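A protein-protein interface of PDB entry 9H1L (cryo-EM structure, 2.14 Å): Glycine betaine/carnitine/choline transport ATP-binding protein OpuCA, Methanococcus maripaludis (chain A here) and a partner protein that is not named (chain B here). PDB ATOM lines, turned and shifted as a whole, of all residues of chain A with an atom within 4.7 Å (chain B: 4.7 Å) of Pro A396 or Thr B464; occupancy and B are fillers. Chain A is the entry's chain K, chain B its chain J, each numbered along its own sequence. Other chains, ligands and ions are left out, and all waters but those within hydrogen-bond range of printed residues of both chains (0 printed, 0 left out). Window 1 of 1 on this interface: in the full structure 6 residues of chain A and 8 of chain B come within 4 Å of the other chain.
Of the printed residues of chain B, Met A395 touches Tyr B447 (3.1 Å). Pro A396 touches three residues of chain B. Printed residues of chain B within 4 Å of Glu A398: Gly B465. Of the printed residues of chain A, Tyr B447 touches Met A395 and Pro A396. Printed residues of chain A within 4 Å of Gly B465: Gly A397 (3.2 Å) and Glu A398 (2.8 Å). Printed residues of chain A within 4 Å of Glu B466: Pro A396. The nearest residue of chain B that does not touch Pro A396 is Gly B465 (4.04 Å). The nearest printed residue of chain A that does not touch Thr B464 is Glu A398 (5.1 Å). The nearest printed residue of chain A that does not touch Gly B465 is Pro A396 (4.04 Å).
Printed residues of chain A that touch a printed residue of chain B: Met A395, Pro A396, Gly A397 and Glu A398. Along chain A the printed residues that touch a printed residue of chain B span positions 395 to 398. Hydrophobic or aromatic side chains of chain B within 4 Å of the printed part of chain A: Tyr B447. Among the printed residues, 6 pairs touch across the chains. Among the printed residues, no Asp or Glu carboxylate lies within 4 Å of a Lys or Arg side-chain nitrogen of the other chain.
Among the printed residues, pairs that only touch across the chains: Pro A396 with Glu B466, Pro A396 with Tyr B447 and Pro A396 with Thr B464.
N of Met A395 lies within hydrogen-bond range of OH of Tyr B447. O of Gly B465 is in hydrogen-bond range of N of Gly A397, 3.2 Å away. The backbone carbonyl oxygen of Gly B465 is in hydrogen-bond range of the backbone NH of Glu A398 (2.8 Å).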
ATOM      1  N   MET A 395      35.331  -2.754  33.115  1.00  0.00           N
ATOM      2  CA  MET A 395      33.943  -2.436  33.413  1.00  0.00           C
ATOM      3  C   MET A 395      33.345  -1.734  32.194  1.00  0.00           C
ATOM      4  O   MET A 395      34.086  -1.168  31.386  1.00  0.00           O
ATOM      5  CB  MET A 395      33.831  -1.551  34.665  1.00  0.00           C
ATOM      6  CG  MET A 395      34.461  -0.180  34.528  1.00  0.00           C
ATOM      7  SD  MET A 395      34.580   0.723  36.089  1.00  0.00           S
ATOM      8  CE  MET A 395      33.430  -0.159  37.136  1.00  0.00           C
ATOM      9  N   PRO A 396      32.021  -1.791  32.028  1.00  0.00           N
ATOM     10  CA  PRO A 396      31.387  -1.047  30.934  1.00  0.00           C
ATOM     11  C   PRO A 396      31.542   0.456  31.112  1.00  0.00           C
ATOM     12  O   PRO A 396      31.707   0.960  32.225  1.00  0.00           O
ATOM     13  CB  PRO A 396      29.918  -1.472  31.019  1.00  0.00           C
ATOM     14  CG  PRO A 396      29.954  -2.801  31.679  1.00  0.00           C
ATOM     15  CD  PRO A 396      31.083  -2.736  32.661  1.00  0.00           C
ATOM     16  N   GLY A 397      31.490   1.171  29.986  1.00  0.00           N
ATOM     17  CA  GLY A 397      31.754   2.601  29.980  1.00  0.00           C
ATOM     18  C   GLY A 397      30.719   3.440  30.700  1.00  0.00           C
ATOM     19  O   GLY A 397      31.021   4.575  31.089  1.00  0.00           O
ATOM     20  N   GLU A 398      29.505   2.917  30.880  1.00  0.00           N
ATOM     21  CA  GLU A 398      28.489   3.660  31.617  1.00  0.00           C
ATOM     22  C   GLU A 398      28.814   3.742  33.105  1.00  0.00           C
ATOM     23  O   GLU A 398      28.512   4.754  33.747  1.00  0.00           O
ATOM     24  CB  GLU A 398      27.117   3.021  31.415  1.00  0.00           C
ATOM     25  CG  GLU A 398      25.958   3.983  31.609  1.00  0.00           C
ATOM     26  CD  GLU A 398      24.623   3.277  31.691  1.00  0.00           C
ATOM     27  OE1 GLU A 398      24.440   2.265  30.980  1.00  0.00           O
ATOM     28  OE2 GLU A 398      23.758   3.733  32.466  1.00  0.00           O
ATOM     29  N   PHE A 399      29.422   2.701  33.663  1.00  0.00           N
ATOM     30  CA  PHE A 399      29.691   2.622  35.089  1.00  0.00           C
ATOM     31  C   PHE A 399      31.116   3.014  35.455  1.00  0.00           C
ATOM     32  O   PHE A 399      31.485   2.926  36.630  1.00  0.00           O
ATOM     33  CB  PHE A 399      29.395   1.208  35.594  1.00  0.00           C
ATOM     34  CG  PHE A 399      28.157   0.614  35.000  1.00  0.00           C
ATOM     35  CD1 PHE A 399      26.910   1.139  35.293  1.00  0.00           C
ATOM     36  CD2 PHE A 399      28.240  -0.459  34.128  1.00  0.00           C
ATOM     37  CE1 PHE A 399      25.767   0.600  34.738  1.00  0.00           C
ATOM     38  CE2 PHE A 399      27.101  -1.002  33.570  1.00  0.00           C
ATOM     39  CZ  PHE A 399      25.863  -0.472  33.876  1.00  0.00           C
ATOM     40  N   ALA A 400      31.928   3.434  34.484  1.00  0.00           N
ATOM     41  CA  ALA A 400      33.288   3.856  34.789  1.00  0.00           C
ATOM     42  C   ALA A 400      33.346   5.273  35.341  1.00  0.00           C
ATOM     43  O   ALA A 400      34.318   5.619  36.024  1.00  0.00           O
ATOM     44  CB  ALA A 400      34.162   3.743  33.541  1.00  0.00           C
ATOM     45  N   MET B 412      21.626  -6.855  31.837  1.00  0.00           N
ATOM     46  CA  MET B 412      22.529  -7.450  30.866  1.00  0.00           C
ATOM     47  C   MET B 412      22.461  -8.968  30.955  1.00  0.00           C
ATOM     48  O   MET B 412      22.380  -9.532  32.051  1.00  0.00           O
ATOM     49  CB  MET B 412      23.968  -6.981  31.087  1.00  0.00           C
ATOM     50  CG  MET B 412      24.178  -5.492  30.886  1.00  0.00           C
ATOM     51  SD  MET B 412      25.913  -5.029  30.715  1.00  0.00           S
ATOM     52  CE  MET B 412      26.732  -6.571  31.112  1.00  0.00           C
ATOM     53  N   ALA B 439      20.198  -5.434  22.359  1.00  0.00           N
ATOM     54  CA  ALA B 439      21.416  -5.091  21.646  1.00  0.00           C
ATOM     55  C   ALA B 439      22.560  -5.973  22.114  1.00  0.00           C
ATOM     56  O   ALA B 439      22.570  -6.461  23.247  1.00  0.00           O
ATOM     57  CB  ALA B 439      21.781  -3.617  21.838  1.00  0.00           C
ATOM     58  N   THR B 441      26.895  -6.003  22.122  1.00  0.00           N
ATOM     59  CA  THR B 441      28.114  -5.231  21.930  1.00  0.00           C
ATOM     60  C   THR B 441      29.020  -5.957  20.944  1.00  0.00           C
ATOM     61  O   THR B 441      29.269  -7.156  21.089  1.00  0.00           O
ATOM     62  CB  THR B 441      28.843  -5.017  23.256  1.00  0.00           C
ATOM     63  OG1 THR B 441      29.789  -6.070  23.454  1.00  0.00           O
ATOM     64  CG2 THR B 441      27.859  -5.033  24.402  1.00  0.00           C
ATOM     65  N   TYR B 447      33.904  -5.976  26.181  1.00  0.00           N
ATOM     66  CA  TYR B 447      32.895  -6.979  26.519  1.00  0.00           C
ATOM     67  C   TYR B 447      32.030  -7.269  25.294  1.00  0.00           C
ATOM     68  O   TYR B 447      30.844  -6.945  25.222  1.00  0.00           O
ATOM     69  CB  TYR B 447      32.068  -6.514  27.710  1.00  0.00           C
ATOM     70  CG  TYR B 447      32.917  -6.285  28.933  1.00  0.00           C
ATOM     71  CD1 TYR B 447      33.463  -7.355  29.623  1.00  0.00           C
ATOM     72  CD2 TYR B 447      33.193  -5.004  29.383  1.00  0.00           C
ATOM     73  CE1 TYR B 447      34.248  -7.160  30.731  1.00  0.00           C
ATOM     74  CE2 TYR B 447      33.981  -4.799  30.495  1.00  0.00           C
ATOM     75  CZ  TYR B 447      34.505  -5.881  31.164  1.00  0.00           C
ATOM     76  OH  TYR B 447      35.289  -5.693  32.273  1.00  0.00           O
ATOM     77  N   TYR B 450      28.137  -9.612  24.941  1.00  0.00           N
ATOM     78  CA  TYR B 450      27.154  -9.477  26.006  1.00  0.00           C
ATOM     79  C   TYR B 450      25.886  -8.820  25.480  1.00  0.00           C
ATOM     80  O   TYR B 450      25.933  -7.800  24.790  1.00  0.00           O
ATOM     81  CB  TYR B 450      27.722  -8.665  27.165  1.00  0.00           C
ATOM     82  CG  TYR B 450      28.549  -9.479  28.130  1.00  0.00           C
ATOM     83  CD1 TYR B 450      27.960 -10.443  28.931  1.00  0.00           C
ATOM     84  CD2 TYR B 450      29.915  -9.280  28.242  1.00  0.00           C
ATOM     85  CE1 TYR B 450      28.710 -11.189  29.813  1.00  0.00           C
ATOM     86  CE2 TYR B 450      30.673 -10.020  29.121  1.00  0.00           C
ATOM     87  CZ  TYR B 450      30.065 -10.974  29.904  1.00  0.00           C
ATOM     88  OH  TYR B 450      30.819 -11.714  30.782  1.00  0.00           O
ATOM     89  N   ILE B 451      24.747  -9.413  25.817  1.00  0.00           N
ATOM     90  CA  ILE B 451      23.446  -8.909  25.402  1.00  0.00           C
ATOM     91  C   ILE B 451      22.814  -8.191  26.584  1.00  0.00           C
ATOM     92  O   ILE B 451      23.078  -8.515  27.747  1.00  0.00           O
ATOM     93  CB  ILE B 451      22.534 -10.046  24.894  1.00  0.00           C
ATOM     94  CG1 ILE B 451      23.332 -11.028  24.036  1.00  0.00           C
ATOM     95  CG2 ILE B 451      21.380  -9.486  24.090  1.00  0.00           C
ATOM     96  CD1 ILE B 451      22.863 -12.459  24.157  1.00  0.00           C
ATOM     97  N   GLY B 452      21.980  -7.202  26.284  1.00  0.00           N
ATOM     98  CA  GLY B 452      21.313  -6.463  27.338  1.00  0.00           C
ATOM     99  C   GLY B 452      20.145  -5.675  26.792  1.00  0.00           C
ATOM    100  O   GLY B 452      19.975  -5.523  25.581  1.00  0.00           O
ATOM    101  N   GLY B 462      24.193   2.662  25.022  1.00  0.00           N
ATOM    102  CA  GLY B 462      23.308   1.614  24.577  1.00  0.00           C
ATOM    103  C   GLY B 462      22.792   0.786  25.733  1.00  0.00           C
ATOM    104  O   GLY B 462      23.079   1.063  26.900  1.00  0.00           O
ATOM    105  N   PRO B 463      22.017  -0.260  25.429  1.00  0.00           N
ATOM    106  CA  PRO B 463      21.445  -1.097  26.493  1.00  0.00           C
ATOM    107  C   PRO B 463      22.471  -1.896  27.282  1.00  0.00           C
ATOM    108  O   PRO B 463      22.085  -2.609  28.212  1.00  0.00           O
ATOM    109  CB  PRO B 463      20.501  -2.037  25.725  1.00  0.00           C
ATOM    110  CG  PRO B 463      20.269  -1.372  24.410  1.00  0.00           C
ATOM    111  CD  PRO B 463      21.539  -0.657  24.098  1.00  0.00           C
ATOM    112  N   THR B 464      23.758  -1.807  26.946  1.00  0.00           N
ATOM    113  CA  THR B 464      24.787  -2.591  27.617  1.00  0.00           C
ATOM    114  C   THR B 464      25.877  -1.728  28.240  1.00  0.00           C
ATOM    115  O   THR B 464      26.926  -2.259  28.620  1.00  0.00           O
ATOM    116  CB  THR B 464      25.416  -3.588  26.643  1.00  0.00           C
ATOM    117  OG1 THR B 464      25.769  -2.907  25.432  1.00  0.00           O
ATOM    118  CG2 THR B 464      24.442  -4.704  26.322  1.00  0.00           C
ATOM    119  N   GLY B 465      25.664  -0.420  28.352  1.00  0.00           N
ATOM    120  CA  GLY B 465      26.643   0.455  28.961  1.00  0.00           C
ATOM    121  C   GLY B 465      27.754   0.918  28.051  1.00  0.00           C
ATOM    122  O   GLY B 465      28.668   1.603  28.520  1.00  0.00           O
ATOM    123  N   GLU B 466      27.713   0.571  26.770  1.00  0.00           N
ATOM    124  CA  GLU B 466      28.713   0.995  25.803  1.00  0.00           C
ATOM    125  C   GLU B 466      28.142   2.091  24.913  1.00  0.00           C
ATOM    126  O   GLU B 466      26.928   2.279  24.812  1.00  0.00           O
ATOM    127  CB  GLU B 466      29.193  -0.185  24.952  1.00  0.00           C
ATOM    128  CG  GLU B 466      29.463  -1.459  25.732  1.00  0.00           C
ATOM    129  CD  GLU B 466      30.793  -1.428  26.456  1.00  0.00           C
ATOM    130  OE1 GLU B 466      31.599  -0.515  26.186  1.00  0.00           O
ATOM    131  OE2 GLU B 466      31.036  -2.323  27.292  1.00  0.00           O
ATOM    132  N   THR B 471      27.822  -0.865  19.834  1.00  0.00           N
ATOM    133  CA  THR B 471      26.573  -1.573  20.074  1.00  0.00           C
ATOM    134  C   THR B 471      25.839  -1.751  18.754  1.00  0.00           C
ATOM    135  O   THR B 471      25.676  -0.787  18.001  1.00  0.00           O
ATOM    136  CB  THR B 471      25.698  -0.805  21.072  1.00  0.00           C
ATOM    137  OG1 THR B 471      26.130  -1.085  22.407  1.00  0.00           O
ATOM    138  CG2 THR B 471      24.237  -1.182  20.922  1.00  0.00           C
